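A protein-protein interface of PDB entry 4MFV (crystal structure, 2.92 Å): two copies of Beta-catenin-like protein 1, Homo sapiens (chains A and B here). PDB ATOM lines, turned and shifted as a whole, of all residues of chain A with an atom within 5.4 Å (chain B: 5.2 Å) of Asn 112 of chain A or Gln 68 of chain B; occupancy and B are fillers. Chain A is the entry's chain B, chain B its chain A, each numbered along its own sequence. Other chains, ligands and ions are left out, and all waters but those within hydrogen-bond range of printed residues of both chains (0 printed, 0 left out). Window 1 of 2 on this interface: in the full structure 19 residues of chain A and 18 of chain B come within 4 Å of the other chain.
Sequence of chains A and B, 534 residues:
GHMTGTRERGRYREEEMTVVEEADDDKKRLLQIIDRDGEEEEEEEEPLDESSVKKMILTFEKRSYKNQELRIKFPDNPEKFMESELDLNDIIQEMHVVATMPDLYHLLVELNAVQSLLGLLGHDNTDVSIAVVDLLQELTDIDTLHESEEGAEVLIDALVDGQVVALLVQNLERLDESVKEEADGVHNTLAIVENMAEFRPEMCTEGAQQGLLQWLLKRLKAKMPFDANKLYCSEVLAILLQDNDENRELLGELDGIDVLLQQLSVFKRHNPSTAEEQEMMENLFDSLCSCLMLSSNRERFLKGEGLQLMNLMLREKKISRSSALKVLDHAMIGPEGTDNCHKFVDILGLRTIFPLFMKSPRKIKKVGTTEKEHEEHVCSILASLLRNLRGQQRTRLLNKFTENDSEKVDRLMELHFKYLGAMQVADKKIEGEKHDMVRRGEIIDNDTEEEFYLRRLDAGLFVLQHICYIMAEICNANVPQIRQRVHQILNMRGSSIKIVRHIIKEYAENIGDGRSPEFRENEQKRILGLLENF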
ATOM      1  N   GLU A  61      18.929 -21.542 -21.309  1.00  0.00           N
ATOM      2  CA  GLU A  61      18.639 -20.550 -20.277  1.00  0.00           C
ATOM      3  C   GLU A  61      19.429 -20.740 -18.986  1.00  0.00           C
ATOM      4  O   GLU A  61      19.924 -19.766 -18.418  1.00  0.00           O
ATOM      5  CB  GLU A  61      17.139 -20.529 -19.970  1.00  0.00           C
ATOM      6  CG  GLU A  61      16.438 -19.247 -20.386  1.00  0.00           C
ATOM      7  CD  GLU A  61      15.452 -18.755 -19.344  1.00  0.00           C
ATOM      8  OE1 GLU A  61      14.576 -17.937 -19.691  1.00  0.00           O
ATOM      9  OE2 GLU A  61      15.554 -19.189 -18.177  1.00  0.00           O
ATOM     10  N   LEU A 107       7.321 -22.053 -29.234  1.00  0.00           N
ATOM     11  CA  LEU A 107       8.179 -22.351 -28.081  1.00  0.00           C
ATOM     12  C   LEU A 107       9.259 -21.277 -27.847  1.00  0.00           C
ATOM     13  O   LEU A 107       9.286 -20.638 -26.801  1.00  0.00           O
ATOM     14  CB  LEU A 107       8.817 -23.737 -28.230  1.00  0.00           C
ATOM     15  CG  LEU A 107       8.114 -24.942 -27.578  1.00  0.00           C
ATOM     16  CD1 LEU A 107       6.609 -24.766 -27.416  1.00  0.00           C
ATOM     17  CD2 LEU A 107       8.421 -26.205 -28.374  1.00  0.00           C
ATOM     18  N   LEU A 108      10.123 -21.054 -28.825  1.00  0.00           N
ATOM     19  CA  LEU A 108      11.196 -20.068 -28.674  1.00  0.00           C
ATOM     20  C   LEU A 108      10.778 -18.697 -28.108  1.00  0.00           C
ATOM     21  O   LEU A 108      11.466 -18.130 -27.243  1.00  0.00           O
ATOM     22  CB  LEU A 108      11.870 -19.847 -30.017  1.00  0.00           C
ATOM     23  CG  LEU A 108      12.985 -20.823 -30.351  1.00  0.00           C
ATOM     24  CD1 LEU A 108      13.147 -20.857 -31.856  1.00  0.00           C
ATOM     25  CD2 LEU A 108      14.289 -20.448 -29.654  1.00  0.00           C
ATOM     26  N   VAL A 109       9.671 -18.157 -28.615  1.00  0.00           N
ATOM     27  CA  VAL A 109       9.278 -16.790 -28.263  1.00  0.00           C
ATOM     28  C   VAL A 109       8.696 -16.734 -26.859  1.00  0.00           C
ATOM     29  O   VAL A 109       9.239 -16.035 -26.001  1.00  0.00           O
ATOM     30  CB  VAL A 109       8.336 -16.112 -29.312  1.00  0.00           C
ATOM     31  CG1 VAL A 109       7.043 -16.881 -29.532  1.00  0.00           C
ATOM     32  CG2 VAL A 109       8.013 -14.679 -28.906  1.00  0.00           C
ATOM     33  N   GLU A 110       7.627 -17.493 -26.620  1.00  0.00           N
ATOM     34  CA  GLU A 110       6.905 -17.437 -25.347  1.00  0.00           C
ATOM     35  C   GLU A 110       7.826 -17.751 -24.188  1.00  0.00           C
ATOM     36  O   GLU A 110       7.748 -17.098 -23.151  1.00  0.00           O
ATOM     37  CB  GLU A 110       5.726 -18.409 -25.345  1.00  0.00           C
ATOM     38  CG  GLU A 110       4.572 -17.948 -26.220  1.00  0.00           C
ATOM     39  CD  GLU A 110       4.210 -18.958 -27.303  1.00  0.00           C
ATOM     40  OE1 GLU A 110       3.811 -20.103 -26.967  1.00  0.00           O
ATOM     41  OE2 GLU A 110       4.334 -18.604 -28.501  1.00  0.00           O
ATOM     42  N   LEU A 111       8.728 -18.709 -24.396  1.00  0.00           N
ATOM     43  CA  LEU A 111       9.663 -19.142 -23.357  1.00  0.00           C
ATOM     44  C   LEU A 111      10.910 -18.249 -23.218  1.00  0.00           C
ATOM     45  O   LEU A 111      11.810 -18.568 -22.447  1.00  0.00           O
ATOM     46  CB  LEU A 111      10.083 -20.588 -23.612  1.00  0.00           C
ATOM     47  CG  LEU A 111       8.996 -21.647 -23.378  1.00  0.00           C
ATOM     48  CD1 LEU A 111       7.618 -21.313 -23.966  1.00  0.00           C
ATOM     49  CD2 LEU A 111       9.503 -22.993 -23.888  1.00  0.00           C
ATOM     50  N   ASN A 112      10.957 -17.147 -23.970  1.00  0.00           N
ATOM     51  CA  ASN A 112      11.984 -16.096 -23.832  1.00  0.00           C
ATOM     52  C   ASN A 112      13.393 -16.464 -24.323  1.00  0.00           C
ATOM     53  O   ASN A 112      14.397 -15.925 -23.854  1.00  0.00           O
ATOM     54  CB  ASN A 112      12.015 -15.551 -22.393  1.00  0.00           C
ATOM     55  CG  ASN A 112      11.091 -14.360 -22.205  1.00  0.00           C
ATOM     56  OD1 ASN A 112      11.550 -13.253 -21.899  1.00  0.00           O
ATOM     57  ND2 ASN A 112       9.785 -14.572 -22.399  1.00  0.00           N
ATOM     58  N   ALA A 113      13.452 -17.361 -25.300  1.00  0.00           N
ATOM     59  CA  ALA A 113      14.716 -17.758 -25.900  1.00  0.00           C
ATOM     60  C   ALA A 113      15.227 -16.581 -26.684  1.00  0.00           C
ATOM     61  O   ALA A 113      16.379 -16.141 -26.524  1.00  0.00           O
ATOM     62  CB  ALA A 113      14.500 -18.937 -26.831  1.00  0.00           C
ATOM     63  N   VAL A 114      14.318 -16.109 -27.540  1.00  0.00           N
ATOM     64  CA  VAL A 114      14.466 -14.930 -28.382  1.00  0.00           C
ATOM     65  C   VAL A 114      15.040 -13.732 -27.641  1.00  0.00           C
ATOM     66  O   VAL A 114      16.067 -13.186 -28.068  1.00  0.00           O
ATOM     67  CB  VAL A 114      13.093 -14.559 -29.002  1.00  0.00           C
ATOM     68  CG1 VAL A 114      12.038 -14.249 -27.925  1.00  0.00           C
ATOM     69  CG2 VAL A 114      13.235 -13.407 -29.985  1.00  0.00           C
ATOM     70  N   GLN A 115      14.396 -13.359 -26.524  1.00  0.00           N
ATOM     71  CA  GLN A 115      14.768 -12.174 -25.761  1.00  0.00           C
ATOM     72  C   GLN A 115      16.168 -12.357 -25.257  1.00  0.00           C
ATOM     73  O   GLN A 115      17.042 -11.561 -25.552  1.00  0.00           O
ATOM     74  CB  GLN A 115      13.850 -11.961 -24.567  1.00  0.00           C
ATOM     75  CG  GLN A 115      12.414 -11.592 -24.909  1.00  0.00           C
ATOM     76  CD  GLN A 115      11.647 -11.053 -23.700  1.00  0.00           C
ATOM     77  OE1 GLN A 115      12.246 -10.604 -22.715  1.00  0.00           O
ATOM     78  NE2 GLN A 115      10.313 -11.101 -23.765  1.00  0.00           N
ATOM     79  N   SER A 116      16.384 -13.433 -24.514  1.00  0.00           N
ATOM     80  CA  SER A 116      17.715 -13.781 -24.050  1.00  0.00           C
ATOM     81  C   SER A 116      18.680 -13.662 -25.214  1.00  0.00           C
ATOM     82  O   SER A 116      19.677 -12.942 -25.126  1.00  0.00           O
ATOM     83  CB  SER A 116      17.720 -15.211 -23.496  1.00  0.00           C
ATOM     84  OG  SER A 116      16.587 -15.430 -22.669  1.00  0.00           O
ATOM     85  N   LEU A 117      18.355 -14.186 -26.379  1.00  0.00           N
ATOM     86  CA  LEU A 117      19.364 -14.272 -27.429  1.00  0.00           C
ATOM     87  C   LEU A 117      19.981 -12.919 -27.789  1.00  0.00           C
ATOM     88  O   LEU A 117      21.178 -12.810 -28.074  1.00  0.00           O
ATOM     89  CB  LEU A 117      18.750 -14.910 -28.659  1.00  0.00           C
ATOM     90  CG  LEU A 117      18.957 -16.417 -28.691  1.00  0.00           C
ATOM     91  CD1 LEU A 117      17.887 -17.087 -29.526  1.00  0.00           C
ATOM     92  CD2 LEU A 117      20.336 -16.736 -29.230  1.00  0.00           C
ATOM     93  N   SER B  64      13.542 -13.835 -11.347  1.00  0.00           N
ATOM     94  CA  SER B  64      13.029 -13.853 -12.703  1.00  0.00           C
ATOM     95  C   SER B  64      13.107 -15.270 -13.277  1.00  0.00           C
ATOM     96  O   SER B  64      12.134 -15.769 -13.876  1.00  0.00           O
ATOM     97  CB  SER B  64      13.833 -12.876 -13.561  1.00  0.00           C
ATOM     98  OG  SER B  64      15.097 -12.620 -12.972  1.00  0.00           O
ATOM     99  N   TYR B  65      14.267 -15.901 -13.059  1.00  0.00           N
ATOM    100  CA  TYR B  65      14.572 -17.271 -13.524  1.00  0.00           C
ATOM    101  C   TYR B  65      13.615 -18.344 -12.965  1.00  0.00           C
ATOM    102  O   TYR B  65      12.964 -19.058 -13.737  1.00  0.00           O
ATOM    103  CB  TYR B  65      16.036 -17.584 -13.196  1.00  0.00           C
ATOM    104  CG  TYR B  65      16.530 -19.001 -13.399  1.00  0.00           C
ATOM    105  CD1 TYR B  65      17.081 -19.410 -14.614  1.00  0.00           C
ATOM    106  CD2 TYR B  65      16.532 -19.912 -12.335  1.00  0.00           C
ATOM    107  CE1 TYR B  65      17.577 -20.695 -14.771  1.00  0.00           C
ATOM    108  CE2 TYR B  65      17.027 -21.198 -12.482  1.00  0.00           C
ATOM    109  CZ  TYR B  65      17.547 -21.588 -13.696  1.00  0.00           C
ATOM    110  OH  TYR B  65      18.036 -22.870 -13.810  1.00  0.00           O
ATOM    111  N   LYS B  66      13.498 -18.449 -11.638  1.00  0.00           N
ATOM    112  CA  LYS B  66      12.549 -19.408 -11.044  1.00  0.00           C
ATOM    113  C   LYS B  66      11.161 -19.170 -11.623  1.00  0.00           C
ATOM    114  O   LYS B  66      10.400 -20.120 -11.820  1.00  0.00           O
ATOM    115  CB  LYS B  66      12.500 -19.343  -9.501  1.00  0.00           C
ATOM    116  CG  LYS B  66      13.757 -19.809  -8.766  1.00  0.00           C
ATOM    117  CD  LYS B  66      14.091 -21.290  -8.965  1.00  0.00           C
ATOM    118  CE  LYS B  66      15.578 -21.560  -8.727  1.00  0.00           C
ATOM    119  NZ  LYS B  66      16.109 -22.809  -9.343  1.00  0.00           N
ATOM    120  N   ASN B  67      10.841 -17.914 -11.923  1.00  0.00           N
ATOM    121  CA  ASN B  67       9.539 -17.611 -12.488  1.00  0.00           C
ATOM    122  C   ASN B  67       9.356 -18.051 -13.919  1.00  0.00           C
ATOM    123  O   ASN B  67       8.307 -18.594 -14.255  1.00  0.00           O
ATOM    124  CB  ASN B  67       9.192 -16.141 -12.431  1.00  0.00           C
ATOM    125  CG  ASN B  67       7.707 -15.924 -12.618  1.00  0.00           C
ATOM    126  OD1 ASN B  67       7.132 -16.272 -13.651  1.00  0.00           O
ATOM    127  ND2 ASN B  67       7.067 -15.403 -11.600  1.00  0.00           N
ATOM    128  N   GLN B  68      10.376 -17.857 -14.743  1.00  0.00           N
ATOM    129  CA  GLN B  68      10.280 -18.210 -16.149  1.00  0.00           C
ATOM    130  C   GLN B  68      10.023 -19.703 -16.263  1.00  0.00           C
ATOM    131  O   GLN B  68       9.260 -20.149 -17.119  1.00  0.00           O
ATOM    132  CB  GLN B  68      11.565 -17.835 -16.887  1.00  0.00           C
ATOM    133  CG  GLN B  68      11.640 -16.374 -17.301  1.00  0.00           C
ATOM    134  CD  GLN B  68      11.243 -16.158 -18.748  1.00  0.00           C
ATOM    135  OE1 GLN B  68      12.015 -16.440 -19.664  1.00  0.00           O
ATOM    136  NE2 GLN B  68      10.033 -15.654 -18.960  1.00  0.00           N
ATOM    137  N   GLU B  69      10.671 -20.475 -15.397  1.00  0.00           N
ATOM    138  CA  GLU B  69      10.545 -21.955 -15.446  1.00  0.00           C
ATOM    139  C   GLU B  69       9.248 -22.479 -14.826  1.00  0.00           C
ATOM    140  O   GLU B  69       8.768 -23.543 -15.217  1.00  0.00           O
ATOM    141  CB  GLU B  69      11.765 -22.666 -14.837  1.00  0.00           C
ATOM    142  CG  GLU B  69      11.837 -22.698 -13.320  1.00  0.00           C
ATOM    143  CD  GLU B  69      13.149 -23.279 -12.811  1.00  0.00           C
ATOM    144  OE1 GLU B  69      13.293 -23.402 -11.576  1.00  0.00           O
ATOM    145  OE2 GLU B  69      14.040 -23.603 -13.635  1.00  0.00           O
ATOM    146  N   LEU B  70       8.704 -21.738 -13.859  1.00  0.00           N
ATOM    147  CA  LEU B  70       7.331 -21.961 -13.355  1.00  0.00           C
ATOM    148  C   LEU B  70       6.243 -21.413 -14.309  1.00  0.00           C
ATOM    149  O   LEU B  70       5.049 -21.699 -14.150  1.00  0.00           O
ATOM    150  CB  LEU B  70       7.167 -21.312 -11.975  1.00  0.00           C
ATOM    151  CG  LEU B  70       7.306 -22.239 -10.768  1.00  0.00           C
ATOM    152  CD1 LEU B  70       8.205 -21.628  -9.697  1.00  0.00           C
ATOM    153  CD2 LEU B  70       5.915 -22.565 -10.222  1.00  0.00           C
ATOM    154  N   ARG B  71       6.670 -20.595 -15.267  1.00  0.00           N
ATOM    155  CA  ARG B  71       5.793 -20.068 -16.299  1.00  0.00           C
ATOM    156  C   ARG B  71       5.768 -21.100 -17.427  1.00  0.00           C
ATOM    157  O   ARG B  71       4.814 -21.168 -18.202  1.00  0.00           O
ATOM    158  CB  ARG B  71       6.298 -18.683 -16.777  1.00  0.00           C
ATOM    159  CG  ARG B  71       5.240 -17.578 -16.869  1.00  0.00           C
ATOM    160  CD  ARG B  71       4.525 -17.290 -15.543  1.00  0.00           C
ATOM    161  NE  ARG B  71       3.657 -16.097 -15.578  1.00  0.00           N
ATOM    162  CZ  ARG B  71       2.460 -16.012 -16.186  1.00  0.00           C
ATOM    163  NH1 ARG B  71       1.945 -17.036 -16.855  1.00  0.00           N
ATOM    164  NH2 ARG B  71       1.761 -14.880 -16.134  1.00  0.00           N
ATOM    165  N   ILE B  72       6.822 -21.907 -17.498  1.00  0.00           N
ATOM    166  CA  ILE B  72       6.899 -23.023 -18.441  1.00  0.00           C
ATOM    167  C   ILE B  72       6.294 -24.337 -17.869  1.00  0.00           C
ATOM    168  O   ILE B  72       5.770 -25.158 -18.633  1.00  0.00           O
ATOM    169  CB  ILE B  72       8.366 -23.274 -18.878  1.00  0.00           C
ATOM    170  CG1 ILE B  72       8.989 -22.004 -19.470  1.00  0.00           C
ATOM    171  CG2 ILE B  72       8.449 -24.403 -19.905  1.00  0.00           C
ATOM    172  CD1 ILE B  72      10.507 -22.044 -19.564  1.00  0.00           C
ATOM    173  N   GLY B 119      12.060  -7.193 -20.352  1.00  0.00           N
ATOM    174  CA  GLY B 119      11.216  -8.356 -20.590  1.00  0.00           C
ATOM    175  C   GLY B 119      10.085  -8.476 -19.583  1.00  0.00           C
ATOM    176  O   GLY B 119       8.995  -9.039 -19.816  1.00  0.00           O
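Of the printed residues of chain B, Glu 61 of chain A touches Tyr 65 (3.9 Å) and Gln 68 (3.0 Å). Printed residues of chain B within 4 Å of Leu 111 of chain A: Gln 68 (3.5 Å) and Ile 72 (3.9 Å). Asn 112 of chain A touches just one residue of chain B: Gln 68 (2.9 Å). Of the printed residues of chain B, Gln 115 of chain A touches Gly 119 (3.3 Å). Printed residues of chain A within 4 Å of Tyr 65 of chain B: Glu 61 (3.9 Å). Gln 68 of chain B touches just these residues of chain A: Glu 61 (3.0 Å), Leu 111 (3.5 Å) and Asn 112 (2.9 Å). Of the printed residues of chain A, Ile 72 of chain B touches Leu 111. The nearest residue of chain A that does not touch Gln 68 of chain B is Glu 110 of chain A (5.0 Å). The nearest printed residue of chain B that does not touch Leu 111 of chain A is Arg 71 of chain B (6.4 Å).
Among the printed residues, merely in contact across the chains: Asn 112 of chain A with Gln 68 of chain B (2.9 Å), Gln 115 of chain A with Gly 119 of chain B (3.3 Å), Leu 111 of chain A with Gln 68 of chain B (3.5 Å), Glu 61 of chain A with Tyr 65 of chain B (3.9 Å) and Leu 111 of chain A with Ile 72 of chain B (3.9 Å).
Printed residues of chain A that touch a printed residue of chain B: Glu 61, Leu 111, Asn 112 and Gln 115. Along chain A the printed residues that touch a printed residue of chain B span positions 61 to 115. Printed residues of chain B that touch a printed residue of chain A: Tyr 65, Gln 68, Ile 72 and Gly 119. Hydrophobic or aromatic side chains of chain B that line the printed part of chain A: Tyr 65 and Ile 72. Among the printed residues, 6 pairs touch across the chains. Among the printed residues, no Asp or Glu carboxylate lies within 4 Å of a Lys or Arg side-chain nitrogen of the other chain.
The side-chain amide oxygen (OE1) of Gln 68 of chain B sits close to the side-chain carboxylate (OE1) of Glu 61 of chain A (3.0 Å).
The side-chain amide nitrogen (ND2) of Asn 112 of chain A sits at hydrogen-bond distance from the backbone carbonyl oxygen (O) of Glu 110 of chain A, 3.3 Å away. O of Asn 112 of chain A is in hydrogen-bond range of OG of Ser 116 of chain A. The side-chain amide oxygen (OD1) of Asn 112 of chain A lies close to the side-chain amide oxygen (OE1) of Gln 115 of chain A (2.9 Å).
No position is printed for both chains. Of the 6 pairs that touch across the chains among the printed residues, none has its exchanged pair printed and touching as well.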
